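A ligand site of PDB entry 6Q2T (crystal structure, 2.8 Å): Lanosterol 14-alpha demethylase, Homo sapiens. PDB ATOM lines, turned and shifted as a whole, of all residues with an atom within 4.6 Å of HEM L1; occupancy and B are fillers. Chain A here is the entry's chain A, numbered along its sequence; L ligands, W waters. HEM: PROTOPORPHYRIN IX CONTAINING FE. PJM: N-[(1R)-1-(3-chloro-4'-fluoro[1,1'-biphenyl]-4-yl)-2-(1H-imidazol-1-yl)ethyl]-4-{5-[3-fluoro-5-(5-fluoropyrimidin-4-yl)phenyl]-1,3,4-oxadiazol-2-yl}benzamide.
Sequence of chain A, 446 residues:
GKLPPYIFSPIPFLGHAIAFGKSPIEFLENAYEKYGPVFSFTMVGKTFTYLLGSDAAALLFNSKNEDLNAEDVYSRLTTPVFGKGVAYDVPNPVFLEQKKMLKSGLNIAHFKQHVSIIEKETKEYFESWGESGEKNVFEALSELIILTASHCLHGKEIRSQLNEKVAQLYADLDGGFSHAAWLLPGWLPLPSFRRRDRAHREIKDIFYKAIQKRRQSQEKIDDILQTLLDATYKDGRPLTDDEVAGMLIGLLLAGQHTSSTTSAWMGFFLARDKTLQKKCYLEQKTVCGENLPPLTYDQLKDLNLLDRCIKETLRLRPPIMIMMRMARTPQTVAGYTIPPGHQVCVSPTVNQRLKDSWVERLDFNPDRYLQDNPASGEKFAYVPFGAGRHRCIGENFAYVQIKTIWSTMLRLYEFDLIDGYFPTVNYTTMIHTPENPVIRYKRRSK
O of Thr 258 is in hydrogen-bond range of OG1 of Thr 262, at 2.5 Å. O of Gly 255 lies within hydrogen-bond range of OG1 of Thr 258 (3.4 Å). The side-chain hydroxyl of Thr 258 lies within hydrogen-bond range of the backbone carbonyl oxygen of Ala 254 (2.5 Å). The backbone carbonyl oxygen of Arg 389 sits at hydrogen-bond distance from the side-chain amino group of Lys 99 (3.0 Å). The backbone NH (N) of Cys 392 sits at hydrogen-bond distance from the backbone carbonyl oxygen (O) of Phe 385, at 2.9 Å. SG of Cys 392 sits close to N of Gly 394 (3.4 Å). NZ of Lys 99 lies within hydrogen-bond range of O of Arg 391. O of Gly 255 sits at hydrogen-bond distance from OG of Ser 259.
NH2 of Arg 325 lies within salt-bridge range of O2A of HEM L1, 2.7 Å away. The side-chain amino group of Lys 99 lies within salt-bridge range of an oxygen (O2D) of HEM L1, at 3.3 Å. ND1 of His 390 sits at hydrogen-bond distance from O1D of HEM L1 (2.7 Å). OH of Tyr 88 is in hydrogen-bond range of O1D of HEM L1 (2.8 Å). The side-chain sulfur (SG) of Cys 392 binds an iron atom (FE) of HEM L1 (2.2 Å).
Merely in contact with HEM L1: Phe 95 (3.1 Å), Pro 384 (3.2 Å), Pro 319 (3.3 Å), Thr 258 (3.3 Å), Gly 255 (3.4 Å), Ala 254 (3.4 Å), Ile 320 (3.5 Å), Met 323 (3.5 Å), Phe 385 (3.6 Å), Leu 251 (3.6 Å), Gly 394 (3.7 Å), Tyr 74 (3.7 Å), Ile 393 (3.7 Å), Gly 386 (3.7 Å), Ala 398 (3.8 Å), Arg 391 (3.9 Å), Phe 397 (3.9 Å) and Leu 314 (3.98 Å). Hydrophobic or aromatic side chains within 4 Å of HEM L1: Tyr 74, Tyr 88, Phe 95, Leu 251, Ala 254, Leu 314, Pro 319, Ile 320, Met 323, Phe 385, His 390, Ile 393, Phe 397 and Ala 398. 23 residues have an atom within 4 Å of HEM L1: Tyr 74, Tyr 88, Phe 95, Lys 99, Leu 251, Ala 254, Gly 255, Thr 258, Leu 314, Pro 319, Ile 320, Met 323, Arg 325, Pro 384, Phe 385, Gly 386, His 390, Arg 391, Cys 392, Ile 393, Gly 394, Phe 397 and Ala 398.
Water W1 lies within hydrogen-bond range of ND1 of His 390 (3.0 Å), O2D of HEM L1 (3.1 Å) and O of Arg 389 (3.2 Å).
An iron atom (FE) of HEM L1 is bound by a nitrogen (NAZ) of PJM L2 (2.1 Å).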
ATOM      1  N   TYR A  74     -20.358   2.064  36.795  1.00  0.00           N
ATOM      2  CA  TYR A  74     -20.560   3.291  35.991  1.00  0.00           C
ATOM      3  C   TYR A  74     -20.025   4.525  36.734  1.00  0.00           C
ATOM      4  O   TYR A  74     -19.480   5.434  36.070  1.00  0.00           O
ATOM      5  CB  TYR A  74     -22.036   3.466  35.614  1.00  0.00           C
ATOM      6  CG  TYR A  74     -22.552   2.433  34.639  1.00  0.00           C
ATOM      7  CD1 TYR A  74     -21.727   1.855  33.689  1.00  0.00           C
ATOM      8  CD2 TYR A  74     -23.886   2.058  34.647  1.00  0.00           C
ATOM      9  CE1 TYR A  74     -22.203   0.915  32.799  1.00  0.00           C
ATOM     10  CE2 TYR A  74     -24.377   1.122  33.750  1.00  0.00           C
ATOM     11  CZ  TYR A  74     -23.531   0.541  32.826  1.00  0.00           C
ATOM     12  OH  TYR A  74     -23.999  -0.386  31.944  1.00  0.00           O
ATOM     13  N   TYR A  88     -25.006   8.289  39.484  1.00  0.00           N
ATOM     14  CA  TYR A  88     -24.389   7.109  40.151  1.00  0.00           C
ATOM     15  C   TYR A  88     -23.545   7.569  41.338  1.00  0.00           C
ATOM     16  O   TYR A  88     -22.960   6.703  42.028  1.00  0.00           O
ATOM     17  CB  TYR A  88     -23.569   6.300  39.140  1.00  0.00           C
ATOM     18  CG  TYR A  88     -24.318   5.939  37.888  1.00  0.00           C
ATOM     19  CD1 TYR A  88     -25.330   4.995  37.912  1.00  0.00           C
ATOM     20  CD2 TYR A  88     -24.035   6.551  36.676  1.00  0.00           C
ATOM     21  CE1 TYR A  88     -26.033   4.651  36.759  1.00  0.00           C
ATOM     22  CE2 TYR A  88     -24.724   6.225  35.519  1.00  0.00           C
ATOM     23  CZ  TYR A  88     -25.727   5.272  35.562  1.00  0.00           C
ATOM     24  OH  TYR A  88     -26.418   4.944  34.436  1.00  0.00           O
ATOM     25  N   PHE A  95     -31.603   8.610  42.800  1.00  0.00           N
ATOM     26  CA  PHE A  95     -31.543   8.671  41.313  1.00  0.00           C
ATOM     27  C   PHE A  95     -32.959   8.485  40.743  1.00  0.00           C
ATOM     28  O   PHE A  95     -33.351   9.268  39.854  1.00  0.00           O
ATOM     29  CB  PHE A  95     -30.580   7.617  40.773  1.00  0.00           C
ATOM     30  CG  PHE A  95     -30.305   7.686  39.290  1.00  0.00           C
ATOM     31  CD1 PHE A  95     -30.379   8.889  38.610  1.00  0.00           C
ATOM     32  CD2 PHE A  95     -29.908   6.559  38.588  1.00  0.00           C
ATOM     33  CE1 PHE A  95     -30.113   8.962  37.254  1.00  0.00           C
ATOM     34  CE2 PHE A  95     -29.642   6.632  37.231  1.00  0.00           C
ATOM     35  CZ  PHE A  95     -29.739   7.824  36.569  1.00  0.00           C
ATOM     36  N   LYS A  99     -35.004  10.942  38.413  1.00  0.00           N
ATOM     37  CA  LYS A  99     -35.491  10.403  37.116  1.00  0.00           C
ATOM     38  C   LYS A  99     -36.947  10.845  36.897  1.00  0.00           C
ATOM     39  O   LYS A  99     -37.278  11.214  35.747  1.00  0.00           O
ATOM     40  CB  LYS A  99     -35.349   8.879  37.069  1.00  0.00           C
ATOM     41  CG  LYS A  99     -33.933   8.379  36.816  1.00  0.00           C
ATOM     42  CD  LYS A  99     -33.852   6.889  36.584  1.00  0.00           C
ATOM     43  CE  LYS A  99     -34.316   6.472  35.208  1.00  0.00           C
ATOM     44  NZ  LYS A  99     -34.321   4.996  35.050  1.00  0.00           N
ATOM     45  N   LEU A 153     -33.907  20.999  25.588  1.00  0.00           N
ATOM     46  CA  LEU A 153     -33.707  20.401  26.939  1.00  0.00           C
ATOM     47  C   LEU A 153     -33.187  21.457  27.921  1.00  0.00           C
ATOM     48  O   LEU A 153     -33.534  21.376  29.113  1.00  0.00           O
ATOM     49  CB  LEU A 153     -32.750  19.210  26.840  1.00  0.00           C
ATOM     50  CG  LEU A 153     -33.243  18.064  25.963  1.00  0.00           C
ATOM     51  CD1 LEU A 153     -32.210  16.938  25.910  1.00  0.00           C
ATOM     52  CD2 LEU A 153     -34.573  17.533  26.451  1.00  0.00           C
ATOM     53  N   LEU A 251     -28.551  15.247  30.669  1.00  0.00           N
ATOM     54  CA  LEU A 251     -29.620  15.448  29.650  1.00  0.00           C
ATOM     55  C   LEU A 251     -28.987  15.564  28.253  1.00  0.00           C
ATOM     56  O   LEU A 251     -29.394  14.797  27.361  1.00  0.00           O
ATOM     57  CB  LEU A 251     -30.415  16.716  29.979  1.00  0.00           C
ATOM     58  CG  LEU A 251     -31.539  16.523  31.006  1.00  0.00           C
ATOM     59  CD1 LEU A 251     -32.036  17.874  31.497  1.00  0.00           C
ATOM     60  CD2 LEU A 251     -32.674  15.707  30.417  1.00  0.00           C
ATOM     61  N   ALA A 254     -26.781  12.423  27.036  1.00  0.00           N
ATOM     62  CA  ALA A 254     -27.786  11.369  26.777  1.00  0.00           C
ATOM     63  C   ALA A 254     -28.422  11.610  25.409  1.00  0.00           C
ATOM     64  O   ALA A 254     -28.301  10.738  24.519  1.00  0.00           O
ATOM     65  CB  ALA A 254     -28.820  11.347  27.868  1.00  0.00           C
ATOM     66  N   GLY A 255     -29.010  12.799  25.222  1.00  0.00           N
ATOM     67  CA  GLY A 255     -29.757  13.193  24.016  1.00  0.00           C
ATOM     68  C   GLY A 255     -28.929  13.020  22.748  1.00  0.00           C
ATOM     69  O   GLY A 255     -29.453  12.433  21.778  1.00  0.00           O
ATOM     70  N   THR A 258     -26.614   9.146  21.287  1.00  0.00           N
ATOM     71  CA  THR A 258     -27.609   8.062  21.090  1.00  0.00           C
ATOM     72  C   THR A 258     -28.417   8.344  19.817  1.00  0.00           C
ATOM     73  O   THR A 258     -28.544   7.425  18.977  1.00  0.00           O
ATOM     74  CB  THR A 258     -28.532   7.910  22.308  1.00  0.00           C
ATOM     75  OG1 THR A 258     -29.053   9.201  22.634  1.00  0.00           O
ATOM     76  CG2 THR A 258     -27.823   7.313  23.501  1.00  0.00           C
ATOM     77  N   SER A 259     -28.925   9.567  19.678  1.00  0.00           N
ATOM     78  CA  SER A 259     -29.815  10.015  18.568  1.00  0.00           C
ATOM     79  C   SER A 259     -29.001  10.241  17.289  1.00  0.00           C
ATOM     80  O   SER A 259     -29.453   9.777  16.215  1.00  0.00           O
ATOM     81  CB  SER A 259     -30.580  11.250  18.944  1.00  0.00           C
ATOM     82  OG  SER A 259     -31.616  10.947  19.873  1.00  0.00           O
ATOM     83  N   THR A 262     -27.829   6.969  15.676  1.00  0.00           N
ATOM     84  CA  THR A 262     -29.084   6.302  15.252  1.00  0.00           C
ATOM     85  C   THR A 262     -29.601   6.975  13.980  1.00  0.00           C
ATOM     86  O   THR A 262     -29.868   6.262  12.993  1.00  0.00           O
ATOM     87  CB  THR A 262     -30.141   6.323  16.366  1.00  0.00           C
ATOM     88  OG1 THR A 262     -29.577   5.685  17.508  1.00  0.00           O
ATOM     89  CG2 THR A 262     -31.425   5.642  15.972  1.00  0.00           C
ATOM     90  N   LEU A 314     -32.746   1.105  15.434  1.00  0.00           N
ATOM     91  CA  LEU A 314     -32.328   0.865  16.839  1.00  0.00           C
ATOM     92  C   LEU A 314     -32.226  -0.642  17.092  1.00  0.00           C
ATOM     93  O   LEU A 314     -31.488  -1.031  18.019  1.00  0.00           O
ATOM     94  CB  LEU A 314     -33.343   1.512  17.792  1.00  0.00           C
ATOM     95  CG  LEU A 314     -33.269   3.042  17.885  1.00  0.00           C
ATOM     96  CD1 LEU A 314     -34.524   3.603  18.526  1.00  0.00           C
ATOM     97  CD2 LEU A 314     -32.034   3.470  18.668  1.00  0.00           C
ATOM     98  N   PRO A 319     -27.496   2.331  19.961  1.00  0.00           N
ATOM     99  CA  PRO A 319     -26.316   3.121  20.290  1.00  0.00           C
ATOM    100  C   PRO A 319     -25.569   2.562  21.511  1.00  0.00           C
ATOM    101  O   PRO A 319     -24.356   2.480  21.473  1.00  0.00           O
ATOM    102  CB  PRO A 319     -26.884   4.525  20.556  1.00  0.00           C
ATOM    103  CG  PRO A 319     -28.307   4.271  21.004  1.00  0.00           C
ATOM    104  CD  PRO A 319     -28.752   3.033  20.257  1.00  0.00           C
ATOM    105  N   ILE A 320     -26.325   2.172  22.550  1.00  0.00           N
ATOM    106  CA  ILE A 320     -25.792   1.507  23.775  1.00  0.00           C
ATOM    107  C   ILE A 320     -25.809  -0.005  23.562  1.00  0.00           C
ATOM    108  O   ILE A 320     -26.877  -0.620  23.779  1.00  0.00           O
ATOM    109  CB  ILE A 320     -26.601   1.930  25.026  1.00  0.00           C
ATOM    110  CG1 ILE A 320     -26.607   3.444  25.204  1.00  0.00           C
ATOM    111  CG2 ILE A 320     -26.084   1.213  26.271  1.00  0.00           C
ATOM    112  CD1 ILE A 320     -27.456   3.917  26.367  1.00  0.00           C
ATOM    113  N   MET A 323     -25.286  -3.062  28.351  1.00  0.00           N
ATOM    114  CA  MET A 323     -25.553  -2.566  29.730  1.00  0.00           C
ATOM    115  C   MET A 323     -25.081  -3.634  30.717  1.00  0.00           C
ATOM    116  O   MET A 323     -25.436  -4.816  30.523  1.00  0.00           O
ATOM    117  CB  MET A 323     -27.044  -2.306  29.941  1.00  0.00           C
ATOM    118  CG  MET A 323     -27.669  -1.424  28.887  1.00  0.00           C
ATOM    119  SD  MET A 323     -28.593  -2.368  27.650  1.00  0.00           S
ATOM    120  CE  MET A 323     -29.854  -3.104  28.689  1.00  0.00           C
ATOM    121  N   ARG A 325     -23.871  -4.705  35.039  1.00  0.00           N
ATOM    122  CA  ARG A 325     -24.034  -4.483  36.498  1.00  0.00           C
ATOM    123  C   ARG A 325     -22.942  -5.268  37.251  1.00  0.00           C
ATOM    124  O   ARG A 325     -22.432  -6.250  36.682  1.00  0.00           O
ATOM    125  CB  ARG A 325     -25.416  -4.938  36.972  1.00  0.00           C
ATOM    126  CG  ARG A 325     -26.562  -4.447  36.094  1.00  0.00           C
ATOM    127  CD  ARG A 325     -26.980  -3.022  36.432  1.00  0.00           C
ATOM    128  NE  ARG A 325     -28.116  -2.596  35.639  1.00  0.00           N
ATOM    129  CZ  ARG A 325     -28.041  -1.850  34.544  1.00  0.00           C
ATOM    130  NH1 ARG A 325     -26.860  -1.431  34.106  1.00  0.00           N
ATOM    131  NH2 ARG A 325     -29.138  -1.519  33.885  1.00  0.00           N
ATOM    132  N   VAL A 383     -34.905  -4.205  23.328  1.00  0.00           N
ATOM    133  CA  VAL A 383     -34.592  -3.424  24.567  1.00  0.00           C
ATOM    134  C   VAL A 383     -33.584  -2.319  24.249  1.00  0.00           C
ATOM    135  O   VAL A 383     -32.706  -2.041  25.059  1.00  0.00           O
ATOM    136  CB  VAL A 383     -34.057  -4.337  25.690  1.00  0.00           C
ATOM    137  CG1 VAL A 383     -35.146  -5.213  26.269  1.00  0.00           C
ATOM    138  CG2 VAL A 383     -32.883  -5.180  25.220  1.00  0.00           C
ATOM    139  N   PRO A 384     -33.727  -1.593  23.121  1.00  0.00           N
ATOM    140  CA  PRO A 384     -32.788  -0.518  22.793  1.00  0.00           C
ATOM    141  C   PRO A 384     -32.859   0.658  23.777  1.00  0.00           C
ATOM    142  O   PRO A 384     -31.970   1.493  23.744  1.00  0.00           O
ATOM    143  CB  PRO A 384     -33.229  -0.080  21.386  1.00  0.00           C
ATOM    144  CG  PRO A 384     -34.700  -0.407  21.354  1.00  0.00           C
ATOM    145  CD  PRO A 384     -34.828  -1.692  22.147  1.00  0.00           C
ATOM    146  N   PHE A 385     -33.902   0.704  24.605  1.00  0.00           N
ATOM    147  CA  PHE A 385     -34.090   1.705  25.688  1.00  0.00           C
ATOM    148  C   PHE A 385     -34.031   0.999  27.056  1.00  0.00           C
ATOM    149  O   PHE A 385     -34.223   1.671  28.087  1.00  0.00           O
ATOM    150  CB  PHE A 385     -35.404   2.461  25.507  1.00  0.00           C
ATOM    151  CG  PHE A 385     -35.450   3.332  24.277  1.00  0.00           C
ATOM    152  CD1 PHE A 385     -35.881   2.826  23.066  1.00  0.00           C
ATOM    153  CD2 PHE A 385     -35.020   4.650  24.324  1.00  0.00           C
ATOM    154  CE1 PHE A 385     -35.911   3.625  21.932  1.00  0.00           C
ATOM    155  CE2 PHE A 385     -35.050   5.449  23.190  1.00  0.00           C
ATOM    156  CZ  PHE A 385     -35.504   4.933  21.997  1.00  0.00           C
ATOM    157  N   GLY A 386     -33.771  -0.308  27.040  1.00  0.00           N
ATOM    158  CA  GLY A 386     -33.580  -1.136  28.248  1.00  0.00           C
ATOM    159  C   GLY A 386     -34.906  -1.462  28.904  1.00  0.00           C
ATOM    160  O   GLY A 386     -35.930  -1.525  28.197  1.00  0.00           O
ATOM    161  N   ARG A 389     -35.458  -0.681  36.528  1.00  0.00           N
ATOM    162  CA  ARG A 389     -35.286   0.565  37.327  1.00  0.00           C
ATOM    163  C   ARG A 389     -34.309   1.503  36.627  1.00  0.00           C
ATOM    164  O   ARG A 389     -34.245   2.691  37.034  1.00  0.00           O
ATOM    165  CB  ARG A 389     -34.791   0.238  38.741  1.00  0.00           C
ATOM    166  CG  ARG A 389     -35.828  -0.448  39.621  1.00  0.00           C
ATOM    167  CD  ARG A 389     -35.214  -1.002  40.899  1.00  0.00           C
ATOM    168  NE  ARG A 389     -36.207  -1.656  41.744  1.00  0.00           N
ATOM    169  CZ  ARG A 389     -36.673  -2.876  41.542  1.00  0.00           C
ATOM    170  NH1 ARG A 389     -36.271  -3.585  40.510  1.00  0.00           N
ATOM    171  NH2 ARG A 389     -37.564  -3.386  42.378  1.00  0.00           N
ATOM    172  N   HIS A 390     -33.560   1.013  35.638  1.00  0.00           N
ATOM    173  CA  HIS A 390     -32.495   1.772  34.920  1.00  0.00           C
ATOM    174  C   HIS A 390     -32.928   2.072  33.482  1.00  0.00           C
ATOM    175  O   HIS A 390     -32.124   2.694  32.752  1.00  0.00           O
ATOM    176  CB  HIS A 390     -31.174   1.002  34.956  1.00  0.00           C
ATOM    177  CG  HIS A 390     -30.501   1.009  36.291  1.00  0.00           C
ATOM    178  ND1 HIS A 390     -29.929   2.146  36.826  1.00  0.00           N
ATOM    179  CD2 HIS A 390     -30.286   0.015  37.185  1.00  0.00           C
ATOM    180  CE1 HIS A 390     -29.411   1.859  38.001  1.00  0.00           C
ATOM    181  NE2 HIS A 390     -29.611   0.557  38.244  1.00  0.00           N
ATOM    182  N   ARG A 391     -34.137   1.655  33.096  1.00  0.00           N
ATOM    183  CA  ARG A 391     -34.677   1.861  31.726  1.00  0.00           C
ATOM    184  C   ARG A 391     -34.595   3.354  31.383  1.00  0.00           C
ATOM    185  O   ARG A 391     -34.463   4.173  32.314  1.00  0.00           O
ATOM    186  CB  ARG A 391     -36.124   1.362  31.629  1.00  0.00           C
ATOM    187  CG  ARG A 391     -37.135   2.248  32.321  1.00  0.00           C
ATOM    188  CD  ARG A 391     -38.554   1.719  32.158  1.00  0.00           C
ATOM    189  NE  ARG A 391     -39.497   2.389  33.048  1.00  0.00           N
ATOM    190  CZ  ARG A 391     -40.795   2.116  33.099  1.00  0.00           C
ATOM    191  NH1 ARG A 391     -41.305   1.190  32.301  1.00  0.00           N
ATOM    192  NH2 ARG A 391     -41.585   2.768  33.939  1.00  0.00           N
ATOM    193  N   CYS A 392     -34.670   3.689  30.085  1.00  0.00           N
ATOM    194  CA  CYS A 392     -34.516   5.066  29.546  1.00  0.00           C
ATOM    195  C   CYS A 392     -35.779   5.885  29.844  1.00  0.00           C
ATOM    196  O   CYS A 392     -36.885   5.330  29.733  1.00  0.00           O
ATOM    197  CB  CYS A 392     -34.253   5.043  28.043  1.00  0.00           C
ATOM    198  SG  CYS A 392     -33.553   6.590  27.415  1.00  0.00           S
ATOM    199  N   ILE A 393     -35.604   7.168  30.191  1.00  0.00           N
ATOM    200  CA  ILE A 393     -36.717   8.145  30.393  1.00  0.00           C
ATOM    201  C   ILE A 393     -36.804   9.052  29.161  1.00  0.00           C
ATOM    202  O   ILE A 393     -37.706   9.911  29.129  1.00  0.00           O
ATOM    203  CB  ILE A 393     -36.511   8.975  31.687  1.00  0.00           C
ATOM    204  CG1 ILE A 393     -35.216   9.783  31.641  1.00  0.00           C
ATOM    205  CG2 ILE A 393     -36.586   8.071  32.921  1.00  0.00           C
ATOM    206  CD1 ILE A 393     -35.076  10.775  32.772  1.00  0.00           C
ATOM    207  N   GLY A 394     -35.897   8.862  28.196  1.00  0.00           N
ATOM    208  CA  GLY A 394     -35.729   9.771  27.051  1.00  0.00           C
ATOM    209  C   GLY A 394     -36.222   9.142  25.753  1.00  0.00           C
ATOM    210  O   GLY A 394     -35.959   9.719  24.685  1.00  0.00           O
ATOM    211  N   PHE A 397     -38.777  11.730  23.850  1.00  0.00           N
ATOM    212  CA  PHE A 397     -38.027  12.901  23.346  1.00  0.00           C
ATOM    213  C   PHE A 397     -37.165  12.478  22.154  1.00  0.00           C
ATOM    214  O   PHE A 397     -37.112  13.201  21.140  1.00  0.00           O
ATOM    215  CB  PHE A 397     -37.152  13.543  24.425  1.00  0.00           C
ATOM    216  CG  PHE A 397     -36.264  14.645  23.900  1.00  0.00           C
ATOM    217  CD1 PHE A 397     -36.770  15.926  23.704  1.00  0.00           C
ATOM    218  CD2 PHE A 397     -34.968  14.380  23.492  1.00  0.00           C
ATOM    219  CE1 PHE A 397     -35.973  16.922  23.172  1.00  0.00           C
ATOM    220  CE2 PHE A 397     -34.175  15.386  22.961  1.00  0.00           C
ATOM    221  CZ  PHE A 397     -34.676  16.656  22.805  1.00  0.00           C
ATOM    222  N   ALA A 398     -36.466  11.340  22.296  1.00  0.00           N
ATOM    223  CA  ALA A 398     -35.602  10.738  21.255  1.00  0.00           C
ATOM    224  C   ALA A 398     -36.391  10.624  19.939  1.00  0.00           C
ATOM    225  O   ALA A 398     -35.961  11.230  18.938  1.00  0.00           O
ATOM    226  CB  ALA A 398     -35.091   9.397  21.705  1.00  0.00           C
HETATM  227  CHA HEM L   1     -31.013   4.850  30.369  1.00  0.00           C
HETATM  228  CHB HEM L   1     -30.964   4.075  25.592  1.00  0.00           C
HETATM  229  CHC HEM L   1     -31.893   8.800  24.817  1.00  0.00           C
HETATM  230  CHD HEM L   1     -31.769   9.574  29.599  1.00  0.00           C
HETATM  231  C1A HEM L   1     -30.927   4.247  29.132  1.00  0.00           C
HETATM  232  C2A HEM L   1     -30.673   2.876  28.936  1.00  0.00           C
HETATM  233  C3A HEM L   1     -30.651   2.664  27.588  1.00  0.00           C
HETATM  234  C4A HEM L   1     -30.893   3.890  26.951  1.00  0.00           C
HETATM  235  CMA HEM L   1     -30.429   1.338  26.909  1.00  0.00           C
HETATM  236  CAA HEM L   1     -30.465   1.841  30.002  1.00  0.00           C
HETATM  237  CBA HEM L   1     -29.028   1.929  30.533  1.00  0.00           C
HETATM  238  CGA HEM L   1     -28.729   0.753  31.430  1.00  0.00           C
HETATM  239  O1A HEM L   1     -27.648   0.712  32.058  1.00  0.00           O
HETATM  240  O2A HEM L   1     -29.558  -0.178  31.550  1.00  0.00           O
HETATM  241  C1B HEM L   1     -31.228   5.322  25.022  1.00  0.00           C
HETATM  242  C2B HEM L   1     -31.345   5.467  23.606  1.00  0.00           C
HETATM  243  C3B HEM L   1     -31.616   6.777  23.364  1.00  0.00           C
HETATM  244  C4B HEM L   1     -31.653   7.432  24.687  1.00  0.00           C
HETATM  245  CMB HEM L   1     -31.208   4.354  22.598  1.00  0.00           C
HETATM  246  CAB HEM L   1     -31.806   7.433  22.057  1.00  0.00           C
HETATM  247  CBB HEM L   1     -31.713   6.732  20.920  1.00  0.00           C
HETATM  248  C1C HEM L   1     -31.945   9.429  26.053  1.00  0.00           C
HETATM  249  C2C HEM L   1     -32.259  10.783  26.255  1.00  0.00           C
HETATM  250  C3C HEM L   1     -32.233  11.005  27.621  1.00  0.00           C
HETATM  251  C4C HEM L   1     -31.890   9.770  28.242  1.00  0.00           C
HETATM  252  CMC HEM L   1     -32.585  11.799  25.182  1.00  0.00           C
HETATM  253  CAC HEM L   1     -32.495  12.268  28.338  1.00  0.00           C
HETATM  254  CBC HEM L   1     -32.895  13.348  27.673  1.00  0.00           C
HETATM  255  C1D HEM L   1     -31.554   8.317  30.142  1.00  0.00           C
HETATM  256  C2D HEM L   1     -31.524   8.144  31.605  1.00  0.00           C
HETATM  257  C3D HEM L   1     -31.295   6.837  31.826  1.00  0.00           C
HETATM  258  C4D HEM L   1     -31.228   6.217  30.502  1.00  0.00           C
HETATM  259  CMD HEM L   1     -31.692   9.220  32.645  1.00  0.00           C
HETATM  260  CAD HEM L   1     -31.233   6.167  33.179  1.00  0.00           C
HETATM  261  CBD HEM L   1     -29.880   5.502  33.436  1.00  0.00           C
HETATM  262  CGD HEM L   1     -29.982   4.673  34.691  1.00  0.00           C
HETATM  263  O1D HEM L   1     -28.982   4.054  35.132  1.00  0.00           O
HETATM  264  O2D HEM L   1     -31.072   4.607  35.313  1.00  0.00           O
HETATM  265  NA  HEM L   1     -31.052   4.864  27.905  1.00  0.00           N
HETATM  266  NB  HEM L   1     -31.419   6.500  25.622  1.00  0.00           N
HETATM  267  NC  HEM L   1     -31.718   8.825  27.262  1.00  0.00           N
HETATM  268  ND  HEM L   1     -31.379   7.143  29.535  1.00  0.00           N
HETATM  269 FE   HEM L   1     -31.363   6.812  27.700  1.00  0.00          FE
HETATM  270  C4  PJM L   2     -16.455  -1.837  28.516  1.00  0.00           C
HETATM  271  C5  PJM L   2     -16.024  -3.126  28.235  1.00  0.00           C
HETATM  272  C6  PJM L   2     -16.135  -3.639  26.939  1.00  0.00           C
HETATM  273  N1  PJM L   2     -16.689  -2.859  25.927  1.00  0.00           N
HETATM  274  N3  PJM L   2     -17.005  -1.088  27.547  1.00  0.00           N
HETATM  275  F5  PJM L   2     -15.476  -3.896  29.206  1.00  0.00           F
HETATM  276  C2  PJM L   2     -17.134  -1.566  26.243  1.00  0.00           C
HETATM  277  CBQ PJM L   2     -16.386  -1.297  29.790  1.00  0.00           C
HETATM  278  CAX PJM L   2     -17.111  -0.150  30.059  1.00  0.00           C
HETATM  279  CAV PJM L   2     -15.636  -1.903  30.807  1.00  0.00           C
HETATM  280  CBI PJM L   2     -15.612  -1.340  32.080  1.00  0.00           C
HETATM  281  FAC PJM L   2     -14.889  -1.935  33.062  1.00  0.00           F
HETATM  282  CAU PJM L   2     -16.340  -0.183  32.350  1.00  0.00           C
HETATM  283  CBP PJM L   2     -17.060   0.426  31.325  1.00  0.00           C
HETATM  284  CBT PJM L   2     -17.794   1.492  31.593  1.00  0.00           C
HETATM  285  OBF PJM L   2     -18.696   1.947  30.787  1.00  0.00           O
HETATM  286  NBD PJM L   2     -17.830   2.141  32.761  1.00  0.00           N
HETATM  287  NBC PJM L   2     -18.636   2.989  32.694  1.00  0.00           N
HETATM  288  CBS PJM L   2     -19.221   2.907  31.497  1.00  0.00           C
HETATM  289  CBN PJM L   2     -20.167   3.705  31.015  1.00  0.00           C
HETATM  290  CAO PJM L   2     -20.311   3.760  29.635  1.00  0.00           C
HETATM  291  CAK PJM L   2     -21.299   4.574  29.080  1.00  0.00           C
HETATM  292  CAN PJM L   2     -21.014   4.442  31.832  1.00  0.00           C
HETATM  293  CAJ PJM L   2     -22.002   5.256  31.276  1.00  0.00           C
HETATM  294  CBL PJM L   2     -22.137   5.315  29.894  1.00  0.00           C
HETATM  295  CBG PJM L   2     -23.086   6.095  29.227  1.00  0.00           C
HETATM  296  OAA PJM L   2     -22.987   6.253  28.012  1.00  0.00           O
HETATM  297  NBE PJM L   2     -24.065   6.655  29.950  1.00  0.00           N
HETATM  298  CBV PJM L   2     -25.104   7.387  29.218  1.00  0.00           C
HETATM  299  CAY PJM L   2     -26.080   6.355  28.679  1.00  0.00           C
HETATM  300  NBW PJM L   2     -27.244   6.984  28.021  1.00  0.00           N
HETATM  301  CAR PJM L   2     -27.337   7.828  27.004  1.00  0.00           C
HETATM  302  CAF PJM L   2     -28.627   8.059  26.790  1.00  0.00           C
HETATM  303  NAZ PJM L   2     -29.333   7.346  27.667  1.00  0.00           N
HETATM  304  CAT PJM L   2     -28.474   6.676  28.421  1.00  0.00           C
HETATM  305  CBR PJM L   2     -25.787   8.284  30.028  1.00  0.00           C
HETATM  306  CBK PJM L   2     -25.802   9.625  29.663  1.00  0.00           C
HETATM  307 CLA  PJM L   2     -24.961  10.163  28.266  1.00  0.00          CL
HETATM  308  CAW PJM L   2     -26.483  10.546  30.440  1.00  0.00           C
HETATM  309  CAQ PJM L   2     -26.472   7.835  31.136  1.00  0.00           C
HETATM  310  CAP PJM L   2     -27.159   8.754  31.925  1.00  0.00           C
HETATM  311  CBO PJM L   2     -27.148  10.095  31.573  1.00  0.00           C
HETATM  312  CBM PJM L   2     -27.843  10.999  32.355  1.00  0.00           C
HETATM  313  CAL PJM L   2     -28.059  12.296  31.902  1.00  0.00           C
HETATM  314  CAH PJM L   2     -28.773  13.180  32.702  1.00  0.00           C
HETATM  315  CBH PJM L   2     -29.263  12.760  33.931  1.00  0.00           C
HETATM  316  FAB PJM L   2     -29.950  13.624  34.714  1.00  0.00           F
HETATM  317  CAI PJM L   2     -29.049  11.462  34.374  1.00  0.00           C
HETATM  318  CAM PJM L   2     -28.344  10.574  33.578  1.00  0.00           C
HETATM  319  O   HOH W   1     -31.637   4.155  38.280  1.00  0.00           O
